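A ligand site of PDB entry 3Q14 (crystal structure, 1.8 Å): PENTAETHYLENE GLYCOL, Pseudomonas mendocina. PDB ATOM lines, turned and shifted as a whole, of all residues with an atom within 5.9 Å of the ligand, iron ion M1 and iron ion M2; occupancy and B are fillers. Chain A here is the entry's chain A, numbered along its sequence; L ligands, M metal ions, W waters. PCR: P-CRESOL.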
ATOM      1  N   ALA A  99      38.432  14.269 -20.611  1.00  0.00           N
ATOM      2  CA  ALA A  99      37.790  15.299 -19.794  1.00  0.00           C
ATOM      3  C   ALA A  99      36.485  14.820 -19.161  1.00  0.00           C
ATOM      4  O   ALA A  99      36.052  15.366 -18.144  1.00  0.00           O
ATOM      5  CB  ALA A  99      37.549  16.548 -20.623  1.00  0.00           C
ATOM      6  N   ILE A 100      35.872  13.797 -19.759  1.00  0.00           N
ATOM      7  CA  ILE A 100      34.480  13.458 -19.465  1.00  0.00           C
ATOM      8  C   ILE A 100      34.267  12.138 -18.738  1.00  0.00           C
ATOM      9  O   ILE A 100      33.482  12.070 -17.794  1.00  0.00           O
ATOM     10  CB  ILE A 100      33.648  13.470 -20.760  1.00  0.00           C
ATOM     11  CG1 ILE A 100      33.618  14.871 -21.363  1.00  0.00           C
ATOM     12  CG2 ILE A 100      32.226  12.932 -20.505  1.00  0.00           C
ATOM     13  CD1 ILE A 100      32.943  15.910 -20.492  1.00  0.00           C
ATOM     14  N   GLY A 103      34.628  11.973 -14.949  1.00  0.00           N
ATOM     15  CA  GLY A 103      33.731  13.001 -14.437  1.00  0.00           C
ATOM     16  C   GLY A 103      32.281  12.543 -14.423  1.00  0.00           C
ATOM     17  O   GLY A 103      31.519  12.870 -13.495  1.00  0.00           O
ATOM     18  N   GLU A 104      31.866  11.811 -15.455  1.00  0.00           N
ATOM     19  CA  GLU A 104      30.540  11.184 -15.459  1.00  0.00           C
ATOM     20  C   GLU A 104      30.410  10.287 -14.245  1.00  0.00           C
ATOM     21  O   GLU A 104      29.395  10.277 -13.567  1.00  0.00           O
ATOM     22  CB  GLU A 104      30.337  10.330 -16.720  1.00  0.00           C
ATOM     23  CG  GLU A 104      30.388  11.128 -18.003  1.00  0.00           C
ATOM     24  CD  GLU A 104      29.024  11.578 -18.466  1.00  0.00           C
ATOM     25  OE1 GLU A 104      28.877  11.837 -19.674  1.00  0.00           O
ATOM     26  OE2 GLU A 104      28.108  11.672 -17.620  1.00  0.00           O
ATOM     27  N   ALA A 107      29.717  12.166 -11.275  1.00  0.00           N
ATOM     28  CA  ALA A 107      28.345  12.649 -11.197  1.00  0.00           C
ATOM     29  C   ALA A 107      27.422  11.636 -10.526  1.00  0.00           C
ATOM     30  O   ALA A 107      26.347  11.998 -10.048  1.00  0.00           O
ATOM     31  CB  ALA A 107      27.813  13.005 -12.594  1.00  0.00           C
ATOM     32  N   GLU A 111      24.374  12.640  -7.845  1.00  0.00           N
ATOM     33  CA  GLU A 111      23.034  12.053  -7.847  1.00  0.00           C
ATOM     34  C   GLU A 111      22.792  11.314  -6.534  1.00  0.00           C
ATOM     35  O   GLU A 111      21.710  11.410  -5.957  1.00  0.00           O
ATOM     36  CB  GLU A 111      22.836  11.141  -9.055  1.00  0.00           C
ATOM     37  CG  GLU A 111      22.826  11.876 -10.394  1.00  0.00           C
ATOM     38  CD  GLU A 111      21.517  12.652 -10.652  1.00  0.00           C
ATOM     39  OE1 GLU A 111      20.538  12.445  -9.922  1.00  0.00           O
ATOM     40  OE2 GLU A 111      21.483  13.462 -11.601  1.00  0.00           O
ATOM     41  N   ASP A 133      22.032   6.427 -14.569  1.00  0.00           N
ATOM     42  CA  ASP A 133      22.395   7.055 -15.829  1.00  0.00           C
ATOM     43  C   ASP A 133      23.888   7.429 -15.854  1.00  0.00           C
ATOM     44  O   ASP A 133      24.558   7.241 -16.849  1.00  0.00           O
ATOM     45  CB  ASP A 133      21.618   8.355 -16.063  1.00  0.00           C
ATOM     46  CG  ASP A 133      20.134   8.146 -16.288  1.00  0.00           C
ATOM     47  OD1 ASP A 133      19.713   7.044 -16.700  1.00  0.00           O
ATOM     48  OD2 ASP A 133      19.395   9.143 -16.090  1.00  0.00           O
ATOM     49  N   GLU A 134      24.384   8.033 -14.786  1.00  0.00           N
ATOM     50  CA  GLU A 134      25.770   8.482 -14.802  1.00  0.00           C
ATOM     51  C   GLU A 134      26.720   7.286 -14.767  1.00  0.00           C
ATOM     52  O   GLU A 134      27.813   7.332 -15.317  1.00  0.00           O
ATOM     53  CB  GLU A 134      26.085   9.466 -13.667  1.00  0.00           C
ATOM     54  CG  GLU A 134      25.204  10.748 -13.638  1.00  0.00           C
ATOM     55  CD  GLU A 134      25.303  11.604 -14.912  1.00  0.00           C
ATOM     56  OE1 GLU A 134      25.948  11.223 -15.907  1.00  0.00           O
ATOM     57  OE2 GLU A 134      24.748  12.716 -14.878  1.00  0.00           O
ATOM     58  N   HIS A 137      26.984   6.333 -18.254  1.00  0.00           N
ATOM     59  CA  HIS A 137      27.803   7.255 -19.026  1.00  0.00           C
ATOM     60  C   HIS A 137      29.276   7.076 -18.768  1.00  0.00           C
ATOM     61  O   HIS A 137      30.067   7.125 -19.690  1.00  0.00           O
ATOM     62  CB  HIS A 137      27.402   8.687 -18.751  1.00  0.00           C
ATOM     63  CG  HIS A 137      25.964   8.960 -19.060  1.00  0.00           C
ATOM     64  ND1 HIS A 137      25.339  10.130 -18.706  1.00  0.00           N
ATOM     65  CD2 HIS A 137      25.035   8.208 -19.701  1.00  0.00           C
ATOM     66  CE1 HIS A 137      24.081  10.092 -19.110  1.00  0.00           C
ATOM     67  NE2 HIS A 137      23.867   8.927 -19.710  1.00  0.00           N
ATOM     68  N   GLN A 141      31.898   5.608 -21.625  1.00  0.00           N
ATOM     69  CA  GLN A 141      32.971   6.468 -22.082  1.00  0.00           C
ATOM     70  C   GLN A 141      34.354   6.028 -21.625  1.00  0.00           C
ATOM     71  O   GLN A 141      35.347   6.639 -21.972  1.00  0.00           O
ATOM     72  CB  GLN A 141      32.647   7.937 -21.755  1.00  0.00           C
ATOM     73  CG  GLN A 141      31.513   8.427 -22.661  1.00  0.00           C
ATOM     74  CD  GLN A 141      30.959   9.763 -22.240  1.00  0.00           C
ATOM     75  OE1 GLN A 141      30.412   9.900 -21.145  1.00  0.00           O
ATOM     76  NE2 GLN A 141      31.093  10.744 -23.111  1.00  0.00           N
ATOM     77  N   TYR A 162      41.696  12.072 -14.575  1.00  0.00           N
ATOM     78  CA  TYR A 162      41.242  12.508 -13.261  1.00  0.00           C
ATOM     79  C   TYR A 162      42.131  11.998 -12.143  1.00  0.00           C
ATOM     80  O   TYR A 162      42.048  12.461 -11.018  1.00  0.00           O
ATOM     81  CB  TYR A 162      39.784  12.101 -13.016  1.00  0.00           C
ATOM     82  CG  TYR A 162      38.755  12.992 -13.693  1.00  0.00           C
ATOM     83  CD1 TYR A 162      38.704  13.120 -15.069  1.00  0.00           C
ATOM     84  CD2 TYR A 162      37.832  13.703 -12.937  1.00  0.00           C
ATOM     85  CE1 TYR A 162      37.761  13.931 -15.684  1.00  0.00           C
ATOM     86  CE2 TYR A 162      36.870  14.527 -13.543  1.00  0.00           C
ATOM     87  CZ  TYR A 162      36.843  14.627 -14.919  1.00  0.00           C
ATOM     88  OH  TYR A 162      35.912  15.429 -15.531  1.00  0.00           O
ATOM     89  N   PHE A 176      34.120  20.181 -11.128  1.00  0.00           N
ATOM     90  CA  PHE A 176      33.160  19.120 -10.803  1.00  0.00           C
ATOM     91  C   PHE A 176      33.089  18.894  -9.303  1.00  0.00           C
ATOM     92  O   PHE A 176      32.020  18.597  -8.767  1.00  0.00           O
ATOM     93  CB  PHE A 176      33.460  17.844 -11.586  1.00  0.00           C
ATOM     94  CG  PHE A 176      33.143  17.963 -13.036  1.00  0.00           C
ATOM     95  CD1 PHE A 176      31.907  18.454 -13.447  1.00  0.00           C
ATOM     96  CD2 PHE A 176      34.092  17.656 -13.998  1.00  0.00           C
ATOM     97  CE1 PHE A 176      31.608  18.587 -14.793  1.00  0.00           C
ATOM     98  CE2 PHE A 176      33.796  17.781 -15.348  1.00  0.00           C
ATOM     99  CZ  PHE A 176      32.559  18.253 -15.743  1.00  0.00           C
ATOM    100  N   ILE A 180      29.408  19.243  -8.247  1.00  0.00           N
ATOM    101  CA  ILE A 180      28.858  17.892  -8.195  1.00  0.00           C
ATOM    102  C   ILE A 180      29.060  17.207  -6.848  1.00  0.00           C
ATOM    103  O   ILE A 180      28.104  16.757  -6.223  1.00  0.00           O
ATOM    104  CB  ILE A 180      29.473  16.961  -9.268  1.00  0.00           C
ATOM    105  CG1 ILE A 180      29.238  17.542 -10.661  1.00  0.00           C
ATOM    106  CG2 ILE A 180      28.893  15.542  -9.139  1.00  0.00           C
ATOM    107  CD1 ILE A 180      29.538  16.527 -11.784  1.00  0.00           C
ATOM    108  N   LEU A 192      24.320  21.355 -10.735  1.00  0.00           N
ATOM    109  CA  LEU A 192      24.554  20.273 -11.660  1.00  0.00           C
ATOM    110  C   LEU A 192      23.342  20.045 -12.566  1.00  0.00           C
ATOM    111  O   LEU A 192      23.422  20.229 -13.769  1.00  0.00           O
ATOM    112  CB  LEU A 192      24.904  18.985 -10.917  1.00  0.00           C
ATOM    113  CG  LEU A 192      24.981  17.729 -11.806  1.00  0.00           C
ATOM    114  CD1 LEU A 192      26.054  17.870 -12.871  1.00  0.00           C
ATOM    115  CD2 LEU A 192      25.250  16.529 -10.915  1.00  0.00           C
ATOM    116  N   PHE A 196      24.378  23.116 -15.196  1.00  0.00           N
ATOM    117  CA  PHE A 196      25.302  22.399 -16.063  1.00  0.00           C
ATOM    118  C   PHE A 196      24.569  21.503 -17.070  1.00  0.00           C
ATOM    119  O   PHE A 196      24.856  21.540 -18.279  1.00  0.00           O
ATOM    120  CB  PHE A 196      26.284  21.585 -15.216  1.00  0.00           C
ATOM    121  CG  PHE A 196      27.352  20.887 -16.018  1.00  0.00           C
ATOM    122  CD1 PHE A 196      28.289  21.612 -16.727  1.00  0.00           C
ATOM    123  CD2 PHE A 196      27.430  19.507 -16.016  1.00  0.00           C
ATOM    124  CE1 PHE A 196      29.283  20.958 -17.454  1.00  0.00           C
ATOM    125  CE2 PHE A 196      28.430  18.857 -16.750  1.00  0.00           C
ATOM    126  CZ  PHE A 196      29.351  19.586 -17.455  1.00  0.00           C
ATOM    127  N   GLU A 197      23.615  20.713 -16.579  1.00  0.00           N
ATOM    128  CA  GLU A 197      23.040  19.639 -17.412  1.00  0.00           C
ATOM    129  C   GLU A 197      21.893  20.080 -18.321  1.00  0.00           C
ATOM    130  O   GLU A 197      21.620  19.414 -19.315  1.00  0.00           O
ATOM    131  CB  GLU A 197      22.609  18.436 -16.575  1.00  0.00           C
ATOM    132  CG  GLU A 197      23.758  17.743 -15.841  1.00  0.00           C
ATOM    133  CD  GLU A 197      23.295  16.545 -15.012  1.00  0.00           C
ATOM    134  OE1 GLU A 197      22.231  16.635 -14.363  1.00  0.00           O
ATOM    135  OE2 GLU A 197      23.990  15.525 -15.020  1.00  0.00           O
ATOM    136  N   THR A 201      25.846  21.037 -21.168  1.00  0.00           N
ATOM    137  CA  THR A 201      26.280  19.764 -21.738  1.00  0.00           C
ATOM    138  C   THR A 201      25.806  19.553 -23.163  1.00  0.00           C
ATOM    139  O   THR A 201      26.440  18.834 -23.934  1.00  0.00           O
ATOM    140  CB  THR A 201      25.896  18.552 -20.895  1.00  0.00           C
ATOM    141  OG1 THR A 201      24.481  18.546 -20.690  1.00  0.00           O
ATOM    142  CG2 THR A 201      26.605  18.576 -19.544  1.00  0.00           C
ATOM    143  N   PHE A 205      27.731  17.345 -26.048  1.00  0.00           N
ATOM    144  CA  PHE A 205      27.151  16.050 -26.409  1.00  0.00           C
ATOM    145  C   PHE A 205      26.229  16.084 -27.643  1.00  0.00           C
ATOM    146  O   PHE A 205      25.920  15.025 -28.216  1.00  0.00           O
ATOM    147  CB  PHE A 205      26.404  15.453 -25.218  1.00  0.00           C
ATOM    148  CG  PHE A 205      27.326  14.998 -24.121  1.00  0.00           C
ATOM    149  CD1 PHE A 205      27.845  15.909 -23.200  1.00  0.00           C
ATOM    150  CD2 PHE A 205      27.692  13.676 -24.037  1.00  0.00           C
ATOM    151  CE1 PHE A 205      28.698  15.479 -22.205  1.00  0.00           C
ATOM    152  CE2 PHE A 205      28.558  13.250 -23.042  1.00  0.00           C
ATOM    153  CZ  PHE A 205      29.050  14.151 -22.121  1.00  0.00           C
ATOM    154  N   ILE A 227      23.739   9.259 -24.978  1.00  0.00           N
ATOM    155  CA  ILE A 227      24.004   9.713 -23.630  1.00  0.00           C
ATOM    156  C   ILE A 227      23.108  10.909 -23.280  1.00  0.00           C
ATOM    157  O   ILE A 227      22.540  10.975 -22.195  1.00  0.00           O
ATOM    158  CB  ILE A 227      25.503  10.028 -23.448  1.00  0.00           C
ATOM    159  CG1 ILE A 227      26.262   8.712 -23.319  1.00  0.00           C
ATOM    160  CG2 ILE A 227      25.749  10.911 -22.221  1.00  0.00           C
ATOM    161  CD1 ILE A 227      27.800   8.867 -23.410  1.00  0.00           C
ATOM    162  N   GLU A 231      20.477  12.477 -20.047  1.00  0.00           N
ATOM    163  CA  GLU A 231      20.689  13.800 -19.466  1.00  0.00           C
ATOM    164  C   GLU A 231      19.378  14.565 -19.505  1.00  0.00           C
ATOM    165  O   GLU A 231      18.991  15.217 -18.535  1.00  0.00           O
ATOM    166  CB  GLU A 231      21.746  14.546 -20.284  1.00  0.00           C
ATOM    167  CG  GLU A 231      22.074  15.945 -19.758  1.00  0.00           C
ATOM    168  CD  GLU A 231      23.154  15.906 -18.696  1.00  0.00           C
ATOM    169  OE1 GLU A 231      24.215  16.540 -18.874  1.00  0.00           O
ATOM    170  OE2 GLU A 231      22.942  15.224 -17.681  1.00  0.00           O
ATOM    171  N   HIS A 234      17.202  13.237 -16.461  1.00  0.00           N
ATOM    172  CA  HIS A 234      17.601  13.514 -15.083  1.00  0.00           C
ATOM    173  C   HIS A 234      17.945  14.975 -14.804  1.00  0.00           C
ATOM    174  O   HIS A 234      17.885  15.415 -13.662  1.00  0.00           O
ATOM    175  CB  HIS A 234      18.685  12.548 -14.554  1.00  0.00           C
ATOM    176  CG  HIS A 234      20.021  12.671 -15.217  1.00  0.00           C
ATOM    177  ND1 HIS A 234      20.620  11.596 -15.844  1.00  0.00           N
ATOM    178  CD2 HIS A 234      20.912  13.677 -15.276  1.00  0.00           C
ATOM    179  CE1 HIS A 234      21.804  11.949 -16.295  1.00  0.00           C
ATOM    180  NE2 HIS A 234      22.013  13.214 -15.963  1.00  0.00           N
HETATM  181  CB  PCR L   1      31.508  15.277 -16.572  1.00  0.00           C
HETATM  182  CG  PCR L   1      30.021  15.145 -16.742  1.00  0.00           C
HETATM  183  CD1 PCR L   1      29.218  14.913 -15.631  1.00  0.00           C
HETATM  184  CE1 PCR L   1      27.848  14.789 -15.783  1.00  0.00           C
HETATM  185  CD2 PCR L   1      29.462  15.276 -17.997  1.00  0.00           C
HETATM  186  CE2 PCR L   1      28.088  15.144 -18.159  1.00  0.00           C
HETATM  187  CZ  PCR L   1      27.287  14.903 -17.053  1.00  0.00           C
HETATM  188  OH  PCR L   1      25.923  14.784 -17.211  1.00  0.00           O
HETATM  189 FE    FE M   1      26.093  11.954 -17.896  1.00  0.00          FE
HETATM  190 FE    FE M   2      24.008  13.995 -16.401  1.00  0.00          FE
HETATM  191  O   HOH W   1      24.195  12.818 -18.023  1.00  0.00           O
HETATM  192  O   HOH W   2      25.519  15.015 -20.603  1.00  0.00           O
HETATM  193  O   HOH W   3      26.474  12.780 -19.818  1.00  0.00           O
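Iron ion M2 is bound by water W1, OE2 of Glu 197, OE2 of Glu 231, OE2 of Glu 134, NE2 of His 234 and OH of the ligand.
Within 4 Å of iron ion M1: Glu 104, Glu 134 and His 137.
OE2 of Glu 104 binds iron ion M1 (2.1 Å). Iron ion M1 is bound by water W1, at 2.1 Å. OE1 of Glu 134 binds iron ion M1 (2.1 Å). Iron ion M1 is bound by water W3, 2.1 Å away. ND1 of His 137 binds iron ion M1 (2.1 Å). Iron ion M1 has five donor atoms within binding distance.
The side-chain carboxylate of Glu 104 sits close to the side-chain amide oxygen of Gln 141. The side-chain hydroxyl (OG1) of Thr 201 is in hydrogen-bond range of the backbone carbonyl oxygen (O) of Glu 197 (3.3 Å). The side-chain hydroxyl (OG1) of Thr 201 sits at hydrogen-bond distance from the side-chain carboxylate (OE1) of Glu 231. The backbone carbonyl oxygen of Ile 227 sits at hydrogen-bond distance from a ring nitrogen (NE2) of His 137, at 3.5 Å. NE2 of His 137 lies close to O of Asp 133, at 3.4 Å. OE1 of Gln 141 lies close to O of His 137 (3.2 Å). ND1 of His 234 sits at hydrogen-bond distance from OD2 of Asp 133, 2.8 Å away. O of Phe 196 lies within hydrogen-bond range of N of Thr 201 (3.1 Å).
Ile 100 touches the ligand. C of Gly 103 touches CB of the ligand (3.6 Å). CB of Ala 107 touches CE1 of the ligand, 3.7 Å away. Phe 176 touches the ligand. Phe 196 touches the ligand (CE2 to CD2, 3.9 Å). CG2 of Thr 201 touches CE2 of the ligand, at 3.99 Å. Hydrophobic or aromatic side chains within 4 Å of the ligand: Ala 107, Phe 176 and Phe 196.
Within 4 Å of iron ion M2: Glu 134, Glu 197, Glu 231 and His 234. Along chain A the residues within 4 Å of iron ion M2 span positions 134 to 234. The nearest printed residue that does not touch iron ion M2 is His 137 (4.7 Å).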
